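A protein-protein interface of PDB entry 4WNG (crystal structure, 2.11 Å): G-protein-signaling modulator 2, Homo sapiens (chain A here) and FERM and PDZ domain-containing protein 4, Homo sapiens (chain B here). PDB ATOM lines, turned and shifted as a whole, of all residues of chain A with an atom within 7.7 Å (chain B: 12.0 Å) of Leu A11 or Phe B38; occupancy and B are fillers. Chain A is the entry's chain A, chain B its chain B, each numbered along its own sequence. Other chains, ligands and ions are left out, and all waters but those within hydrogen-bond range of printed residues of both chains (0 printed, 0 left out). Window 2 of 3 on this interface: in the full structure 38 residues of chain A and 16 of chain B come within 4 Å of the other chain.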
ATOM      1  N   SER A   5      -5.194   8.774   8.465  1.00  0.00           N
ATOM      2  CA  SER A   5      -5.352   9.845   7.490  1.00  0.00           C
ATOM      3  C   SER A   5      -4.617  11.106   7.962  1.00  0.00           C
ATOM      4  O   SER A   5      -4.105  11.162   9.084  1.00  0.00           O
ATOM      5  CB  SER A   5      -6.842  10.136   7.266  1.00  0.00           C
ATOM      6  OG  SER A   5      -7.557  10.127   8.490  1.00  0.00           O
ATOM      7  N   MET A   6      -4.555  12.107   7.089  1.00  0.00           N
ATOM      8  CA  MET A   6      -4.083  13.435   7.467  1.00  0.00           C
ATOM      9  C   MET A   6      -5.018  14.011   8.525  1.00  0.00           C
ATOM     10  O   MET A   6      -4.581  14.689   9.448  1.00  0.00           O
ATOM     11  CB  MET A   6      -4.076  14.363   6.252  1.00  0.00           C
ATOM     12  CG  MET A   6      -3.134  13.953   5.128  1.00  0.00           C
ATOM     13  SD  MET A   6      -1.574  14.863   5.130  1.00  0.00           S
ATOM     14  CE  MET A   6      -0.575  13.839   6.196  1.00  0.00           C
ATOM     15  N   GLU A   7      -6.312  13.734   8.372  1.00  0.00           N
ATOM     16  CA  GLU A   7      -7.340  14.201   9.306  1.00  0.00           C
ATOM     17  C   GLU A   7      -7.029  13.725  10.721  1.00  0.00           C
ATOM     18  O   GLU A   7      -7.184  14.480  11.679  1.00  0.00           O
ATOM     19  CB  GLU A   7      -8.742  13.688   8.923  1.00  0.00           C
ATOM     20  CG  GLU A   7      -9.028  13.484   7.433  1.00  0.00           C
ATOM     21  CD  GLU A   7      -8.826  14.737   6.602  1.00  0.00           C
ATOM     22  OE1 GLU A   7      -9.753  15.565   6.557  1.00  0.00           O
ATOM     23  OE2 GLU A   7      -7.753  14.880   5.972  1.00  0.00           O
ATOM     24  N   ALA A   8      -6.585  12.472  10.844  1.00  0.00           N
ATOM     25  CA  ALA A   8      -6.390  11.857  12.159  1.00  0.00           C
ATOM     26  C   ALA A   8      -5.196  12.438  12.910  1.00  0.00           C
ATOM     27  O   ALA A   8      -5.299  12.709  14.108  1.00  0.00           O
ATOM     28  CB  ALA A   8      -6.273  10.340  12.036  1.00  0.00           C
ATOM     29  N   SER A   9      -4.079  12.653  12.212  1.00  0.00           N
ATOM     30  CA  SER A   9      -2.896  13.290  12.823  1.00  0.00           C
ATOM     31  C   SER A   9      -3.151  14.753  13.223  1.00  0.00           C
ATOM     32  O   SER A   9      -2.615  15.233  14.226  1.00  0.00           O
ATOM     33  CB  SER A   9      -1.700  13.255  11.871  1.00  0.00           C
ATOM     34  OG  SER A   9      -1.636  12.037  11.172  1.00  0.00           O
ATOM     35  N   CYS A  10      -3.931  15.472  12.417  1.00  0.00           N
ATOM     36  CA  CYS A  10      -4.264  16.867  12.741  1.00  0.00           C
ATOM     37  C   CYS A  10      -4.998  16.941  14.073  1.00  0.00           C
ATOM     38  O   CYS A  10      -4.684  17.751  14.933  1.00  0.00           O
ATOM     39  CB  CYS A  10      -5.122  17.484  11.641  1.00  0.00           C
ATOM     40  SG  CYS A  10      -5.617  19.188  11.989  1.00  0.00           S
ATOM     41  N   LEU A  11      -5.971  16.059  14.230  1.00  0.00           N
ATOM     42  CA  LEU A  11      -6.727  15.945  15.460  1.00  0.00           C
ATOM     43  C   LEU A  11      -5.797  15.682  16.644  1.00  0.00           C
ATOM     44  O   LEU A  11      -5.856  16.389  17.658  1.00  0.00           O
ATOM     45  CB  LEU A  11      -7.734  14.808  15.304  1.00  0.00           C
ATOM     46  CG  LEU A  11      -9.143  14.942  15.859  1.00  0.00           C
ATOM     47  CD1 LEU A  11      -9.745  16.312  15.583  1.00  0.00           C
ATOM     48  CD2 LEU A  11      -9.994  13.845  15.232  1.00  0.00           C
ATOM     49  N   GLU A  12      -4.919  14.689  16.494  1.00  0.00           N
ATOM     50  CA  GLU A  12      -4.001  14.272  17.571  1.00  0.00           C
ATOM     51  C   GLU A  12      -3.109  15.414  18.018  1.00  0.00           C
ATOM     52  O   GLU A  12      -2.973  15.683  19.210  1.00  0.00           O
ATOM     53  CB  GLU A  12      -3.135  13.092  17.108  1.00  0.00           C
ATOM     54  CG  GLU A  12      -3.915  11.794  16.905  1.00  0.00           C
ATOM     55  CD  GLU A  12      -3.053  10.624  16.417  1.00  0.00           C
ATOM     56  OE1 GLU A  12      -1.874  10.842  16.023  1.00  0.00           O
ATOM     57  OE2 GLU A  12      -3.568   9.478  16.427  1.00  0.00           O
ATOM     58  N   LEU A  13      -2.504  16.096  17.053  1.00  0.00           N
ATOM     59  CA  LEU A  13      -1.696  17.279  17.344  1.00  0.00           C
ATOM     60  C   LEU A  13      -2.499  18.338  18.080  1.00  0.00           C
ATOM     61  O   LEU A  13      -2.005  18.981  19.011  1.00  0.00           O
ATOM     62  CB  LEU A  13      -1.160  17.878  16.042  1.00  0.00           C
ATOM     63  CG  LEU A  13      -0.143  17.025  15.283  1.00  0.00           C
ATOM     64  CD1 LEU A  13       0.217  17.692  13.965  1.00  0.00           C
ATOM     65  CD2 LEU A  13       1.090  16.810  16.142  1.00  0.00           C
ATOM     66  N   ALA A  14      -3.741  18.520  17.655  1.00  0.00           N
ATOM     67  CA  ALA A  14      -4.584  19.551  18.226  1.00  0.00           C
ATOM     68  C   ALA A  14      -4.932  19.197  19.662  1.00  0.00           C
ATOM     69  O   ALA A  14      -4.920  20.058  20.528  1.00  0.00           O
ATOM     70  CB  ALA A  14      -5.841  19.740  17.387  1.00  0.00           C
ATOM     71  N   LEU A  15      -5.216  17.921  19.920  1.00  0.00           N
ATOM     72  CA  LEU A  15      -5.510  17.475  21.291  1.00  0.00           C
ATOM     73  C   LEU A  15      -4.353  17.731  22.235  1.00  0.00           C
ATOM     74  O   LEU A  15      -4.549  18.152  23.356  1.00  0.00           O
ATOM     75  CB  LEU A  15      -5.851  15.992  21.331  1.00  0.00           C
ATOM     76  CG  LEU A  15      -7.314  15.614  21.248  1.00  0.00           C
ATOM     77  CD1 LEU A  15      -7.409  14.095  21.283  1.00  0.00           C
ATOM     78  CD2 LEU A  15      -8.101  16.224  22.398  1.00  0.00           C
ATOM     79  N   GLU A  16      -3.144  17.471  21.762  1.00  0.00           N
ATOM     80  CA  GLU A  16      -1.948  17.768  22.530  1.00  0.00           C
ATOM     81  C   GLU A  16      -1.807  19.268  22.737  1.00  0.00           C
ATOM     82  O   GLU A  16      -1.428  19.729  23.812  1.00  0.00           O
ATOM     83  CB  GLU A  16      -0.737  17.179  21.808  1.00  0.00           C
ATOM     84  CG  GLU A  16       0.588  17.317  22.525  1.00  0.00           C
ATOM     85  CD  GLU A  16       0.657  16.582  23.850  1.00  0.00           C
ATOM     86  OE1 GLU A  16      -0.293  15.830  24.199  1.00  0.00           O
ATOM     87  OE2 GLU A  16       1.695  16.758  24.534  1.00  0.00           O
ATOM     88  N   GLY A  17      -2.127  20.043  21.703  1.00  0.00           N
ATOM     89  CA  GLY A  17      -2.158  21.490  21.850  1.00  0.00           C
ATOM     90  C   GLY A  17      -3.103  21.921  22.953  1.00  0.00           C
ATOM     91  O   GLY A  17      -2.730  22.697  23.824  1.00  0.00           O
ATOM     92  N   GLU A  18      -4.330  21.418  22.917  1.00  0.00           N
ATOM     93  CA  GLU A  18      -5.315  21.770  23.953  1.00  0.00           C
ATOM     94  C   GLU A  18      -4.864  21.329  25.330  1.00  0.00           C
ATOM     95  O   GLU A  18      -5.068  22.046  26.295  1.00  0.00           O
ATOM     96  CB  GLU A  18      -6.667  21.135  23.674  1.00  0.00           C
ATOM     97  CG  GLU A  18      -7.219  21.498  22.318  1.00  0.00           C
ATOM     98  CD  GLU A  18      -8.668  21.151  22.165  1.00  0.00           C
ATOM     99  OE1 GLU A  18      -9.171  21.258  21.018  1.00  0.00           O
ATOM    100  OE2 GLU A  18      -9.298  20.781  23.183  1.00  0.00           O
ATOM    101  N   PHE A  33      -0.486  23.495  17.904  1.00  0.00           N
ATOM    102  CA  PHE A  33      -1.586  23.987  17.075  1.00  0.00           C
ATOM    103  C   PHE A  33      -1.036  24.405  15.693  1.00  0.00           C
ATOM    104  O   PHE A  33      -1.663  24.161  14.683  1.00  0.00           O
ATOM    105  CB  PHE A  33      -2.306  25.168  17.743  1.00  0.00           C
ATOM    106  CG  PHE A  33      -3.177  24.797  18.921  1.00  0.00           C
ATOM    107  CD1 PHE A  33      -4.130  23.799  18.828  1.00  0.00           C
ATOM    108  CD2 PHE A  33      -3.080  25.505  20.111  1.00  0.00           C
ATOM    109  CE1 PHE A  33      -4.935  23.488  19.909  1.00  0.00           C
ATOM    110  CE2 PHE A  33      -3.891  25.201  21.190  1.00  0.00           C
ATOM    111  CZ  PHE A  33      -4.816  24.191  21.091  1.00  0.00           C
ATOM    112  N   ALA A  36      -0.438  21.338  13.804  1.00  0.00           N
ATOM    113  CA  ALA A  36      -1.706  20.810  13.302  1.00  0.00           C
ATOM    114  C   ALA A  36      -2.210  21.569  12.068  1.00  0.00           C
ATOM    115  O   ALA A  36      -2.807  20.983  11.158  1.00  0.00           O
ATOM    116  CB  ALA A  36      -2.751  20.870  14.383  1.00  0.00           C
ATOM    117  N   VAL A  39      -0.091  20.305   9.130  1.00  0.00           N
ATOM    118  CA  VAL A  39      -0.548  18.988   8.624  1.00  0.00           C
ATOM    119  C   VAL A  39      -1.818  19.144   7.816  1.00  0.00           C
ATOM    120  O   VAL A  39      -1.959  18.557   6.751  1.00  0.00           O
ATOM    121  CB  VAL A  39      -0.835  18.003   9.780  1.00  0.00           C
ATOM    122  CG1 VAL A  39      -1.599  16.770   9.309  1.00  0.00           C
ATOM    123  CG2 VAL A  39       0.459  17.600  10.462  1.00  0.00           C
ATOM    124  N   GLY A  40      -2.760  19.907   8.367  1.00  0.00           N
ATOM    125  CA  GLY A  40      -4.002  20.233   7.687  1.00  0.00           C
ATOM    126  C   GLY A  40      -5.087  19.197   7.877  1.00  0.00           C
ATOM    127  O   GLY A  40      -4.840  18.107   8.398  1.00  0.00           O
ATOM    128  N   THR A  41      -6.296  19.573   7.453  1.00  0.00           N
ATOM    129  CA  THR A  41      -7.491  18.745   7.526  1.00  0.00           C
ATOM    130  C   THR A  41      -8.548  19.356   6.614  1.00  0.00           C
ATOM    131  O   THR A  41      -8.528  20.559   6.361  1.00  0.00           O
ATOM    132  CB  THR A  41      -8.061  18.660   8.963  1.00  0.00           C
ATOM    133  OG1 THR A  41      -9.359  18.052   8.933  1.00  0.00           O
ATOM    134  CG2 THR A  41      -8.205  20.032   9.587  1.00  0.00           C
ATOM    135  N   ASP A  43     -11.714  19.140   7.439  1.00  0.00           N
ATOM    136  CA  ASP A  43     -12.790  19.517   8.336  1.00  0.00           C
ATOM    137  C   ASP A  43     -12.562  20.946   8.812  1.00  0.00           C
ATOM    138  O   ASP A  43     -11.667  21.211   9.613  1.00  0.00           O
ATOM    139  CB  ASP A  43     -12.872  18.562   9.527  1.00  0.00           C
ATOM    140  CG  ASP A  43     -14.116  18.790  10.377  1.00  0.00           C
ATOM    141  OD1 ASP A  43     -15.188  19.104   9.818  1.00  0.00           O
ATOM    142  OD2 ASP A  43     -14.024  18.646  11.612  1.00  0.00           O
ATOM    143  N   THR A  46     -12.991  21.700  12.650  1.00  0.00           N
ATOM    144  CA  THR A  46     -11.790  21.429  13.434  1.00  0.00           C
ATOM    145  C   THR A  46     -10.792  22.546  13.273  1.00  0.00           C
ATOM    146  O   THR A  46     -10.191  22.990  14.232  1.00  0.00           O
ATOM    147  CB  THR A  46     -11.135  20.105  12.994  1.00  0.00           C
ATOM    148  OG1 THR A  46     -12.011  19.029  13.314  1.00  0.00           O
ATOM    149  CG2 THR A  46      -9.815  19.869  13.704  1.00  0.00           C
ATOM    150  N   LEU A  47     -10.627  23.001  12.042  1.00  0.00           N
ATOM    151  CA  LEU A  47      -9.665  24.056  11.724  1.00  0.00           C
ATOM    152  C   LEU A  47     -10.052  25.371  12.404  1.00  0.00           C
ATOM    153  O   LEU A  47      -9.203  26.098  12.915  1.00  0.00           O
ATOM    154  CB  LEU A  47      -9.601  24.225  10.205  1.00  0.00           C
ATOM    155  CG  LEU A  47      -8.325  24.688   9.520  1.00  0.00           C
ATOM    156  CD1 LEU A  47      -7.081  23.971  10.009  1.00  0.00           C
ATOM    157  CD2 LEU A  47      -8.495  24.479   8.021  1.00  0.00           C
ATOM    158  N   ILE A  50      -9.038  25.215  15.932  1.00  0.00           N
ATOM    159  CA  ILE A  50      -7.590  25.397  16.078  1.00  0.00           C
ATOM    160  C   ILE A  50      -7.204  26.875  15.973  1.00  0.00           C
ATOM    161  O   ILE A  50      -6.422  27.379  16.785  1.00  0.00           O
ATOM    162  CB  ILE A  50      -6.816  24.534  15.059  1.00  0.00           C
ATOM    163  CG1 ILE A  50      -6.994  23.036  15.390  1.00  0.00           C
ATOM    164  CG2 ILE A  50      -5.344  24.924  15.046  1.00  0.00           C
ATOM    165  CD1 ILE A  50      -6.750  22.095  14.229  1.00  0.00           C
ATOM    166  N   LYS B  32     -13.096  27.279  21.970  1.00  0.00           N
ATOM    167  CA  LYS B  32     -13.533  26.192  21.102  1.00  0.00           C
ATOM    168  C   LYS B  32     -12.580  25.027  21.326  1.00  0.00           C
ATOM    169  O   LYS B  32     -11.420  25.227  21.705  1.00  0.00           O
ATOM    170  CB  LYS B  32     -13.493  26.636  19.635  1.00  0.00           C
ATOM    171  CG  LYS B  32     -14.493  27.739  19.316  1.00  0.00           C
ATOM    172  CD  LYS B  32     -14.551  28.071  17.833  1.00  0.00           C
ATOM    173  CE  LYS B  32     -15.216  29.430  17.642  1.00  0.00           C
ATOM    174  NZ  LYS B  32     -15.436  29.783  16.226  1.00  0.00           N
ATOM    175  N   SER B  33     -13.056  23.817  21.096  1.00  0.00           N
ATOM    176  CA  SER B  33     -12.196  22.642  21.182  1.00  0.00           C
ATOM    177  C   SER B  33     -12.487  21.728  20.016  1.00  0.00           C
ATOM    178  O   SER B  33     -13.611  21.703  19.509  1.00  0.00           O
ATOM    179  CB  SER B  33     -12.419  21.911  22.509  1.00  0.00           C
ATOM    180  OG  SER B  33     -11.713  20.682  22.552  1.00  0.00           O
ATOM    181  N   VAL B  34     -11.467  20.981  19.591  1.00  0.00           N
ATOM    182  CA  VAL B  34     -11.641  19.963  18.556  1.00  0.00           C
ATOM    183  C   VAL B  34     -12.534  18.811  19.026  1.00  0.00           C
ATOM    184  O   VAL B  34     -13.138  18.124  18.202  1.00  0.00           O
ATOM    185  CB  VAL B  34     -10.287  19.422  18.019  1.00  0.00           C
ATOM    186  CG1 VAL B  34      -9.484  20.552  17.388  1.00  0.00           C
ATOM    187  CG2 VAL B  34      -9.474  18.723  19.105  1.00  0.00           C
ATOM    188  N   THR B  35     -12.650  18.634  20.339  1.00  0.00           N
ATOM    189  CA  THR B  35     -13.514  17.579  20.913  1.00  0.00           C
ATOM    190  C   THR B  35     -15.013  17.912  20.872  1.00  0.00           C
ATOM    191  O   THR B  35     -15.843  17.034  21.121  1.00  0.00           O
ATOM    192  CB  THR B  35     -13.132  17.247  22.376  1.00  0.00           C
ATOM    193  OG1 THR B  35     -13.417  18.370  23.227  1.00  0.00           O
ATOM    194  CG2 THR B  35     -11.651  16.869  22.480  1.00  0.00           C
ATOM    195  N   ASP B  36     -15.356  19.170  20.580  1.00  0.00           N
ATOM    196  CA  ASP B  36     -16.747  19.549  20.292  1.00  0.00           C
ATOM    197  C   ASP B  36     -17.328  18.633  19.221  1.00  0.00           C
ATOM    198  O   ASP B  36     -16.685  18.377  18.200  1.00  0.00           O
ATOM    199  CB  ASP B  36     -16.849  20.996  19.769  1.00  0.00           C
ATOM    200  CG  ASP B  36     -16.518  22.041  20.819  1.00  0.00           C
ATOM    201  OD1 ASP B  36     -16.524  21.703  22.024  1.00  0.00           O
ATOM    202  OD2 ASP B  36     -16.255  23.206  20.427  1.00  0.00           O
ATOM    203  N   TYR B  37     -18.538  18.138  19.464  1.00  0.00           N
ATOM    204  CA  TYR B  37     -19.314  17.417  18.451  1.00  0.00           C
ATOM    205  C   TYR B  37     -18.688  16.098  17.948  1.00  0.00           C
ATOM    206  O   TYR B  37     -18.913  15.710  16.798  1.00  0.00           O
ATOM    207  CB  TYR B  37     -19.612  18.345  17.264  1.00  0.00           C
ATOM    208  N   PHE B  38     -17.910  15.423  18.800  1.00  0.00           N
ATOM    209  CA  PHE B  38     -17.534  14.013  18.560  1.00  0.00           C
ATOM    210  C   PHE B  38     -16.860  13.363  19.777  1.00  0.00           C
ATOM    211  O   PHE B  38     -16.021  13.967  20.446  1.00  0.00           O
ATOM    212  CB  PHE B  38     -16.682  13.845  17.278  1.00  0.00           C
ATOM    213  CG  PHE B  38     -15.195  13.969  17.487  1.00  0.00           C
ATOM    214  CD1 PHE B  38     -14.446  12.872  17.897  1.00  0.00           C
ATOM    215  CD2 PHE B  38     -14.536  15.163  17.228  1.00  0.00           C
ATOM    216  CE1 PHE B  38     -13.079  12.972  18.076  1.00  0.00           C
ATOM    217  CE2 PHE B  38     -13.166  15.265  17.402  1.00  0.00           C
ATOM    218  CZ  PHE B  38     -12.438  14.171  17.831  1.00  0.00           C
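The side-chain hydroxyl (OG) of Ser B33 is in hydrogen-bond range of the side-chain carboxylate (OE2) of Glu A18 (2.5 Å). OE1 of Glu A18 is in hydrogen-bond range of N of Val B34 (2.7 Å).
Printed residues of chain B that touch a printed residue of chain A: Ser B33, Val B34, Thr B35 and Phe B38. Of the 23 printed residues of chain A, 5 touch a printed residue of chain B. Hydrophobic or aromatic side chains of chain A within 4 Å of the printed part of chain B: Leu A11, Ala A14 and Leu A15. Among the printed residues, 7 pairs touch across the chains.
CD1 of Leu A11 touches CB of Val B34, 3.99 Å away. Leu A11 touches Phe B38 (CD2 to CZ, 3.6 Å). Val B34 touches Ala A14. Thr B35 touches Leu A15 (CG2 to CD2, 3.6 Å). CG2 of Thr A46 touches CG1 of Val B34, 3.8 Å away.
The side-chain hydroxyl (OG1) of Thr B35 is in hydrogen-bond range of the side-chain hydroxyl (OG) of Ser B33 (3.0 Å). The side-chain hydroxyl of Thr A46 is in hydrogen-bond range of the side-chain carboxylate of Asp A43, at 2.7 Å. The side-chain carboxylate (OD2) of Asp B36 sits at hydrogen-bond distance from the backbone NH (N) of Ser B33 (3.3 Å).
No residue of chain B comes within 4 Å of Ala A8. No residue of chain B comes within 4 Å of Ser A9. Printed residues of chain B within 4 Å of Leu A11: Val B34 and Phe B38. No residue of chain B comes within 4 Å of Glu A12. No residue of chain B comes within 4 Å of Leu A13. Of the printed residues of chain B, Ala A14 touches Val B34. Of the printed residues of chain B, Glu A18 touches Ser B33 (2.5 Å) and Val B34 (2.7 Å). Ala A36 touches none of the printed residues of chain B. Of chain B, only Val B34 (3.8 Å) comes within 4 Å of Thr A46. Lys B32 touches none of the printed residues of chain A. Of the printed residues of chain A, Ser B33 touches Glu A18 (2.5 Å). Of the printed residues of chain A, Val B34 touches Leu A11 (3.99 Å), Ala A14 (3.7 Å), Glu A18 (2.7 Å) and Thr A46 (3.8 Å). Of the printed residues of chain A, Thr B35 touches Leu A15. Tyr B37 touches none of the printed residues of chain A. Phe B38 touches one residue of chain A. The nearest printed residue of chain B that does not touch Glu A18 is Thr B35 (4.4 Å).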
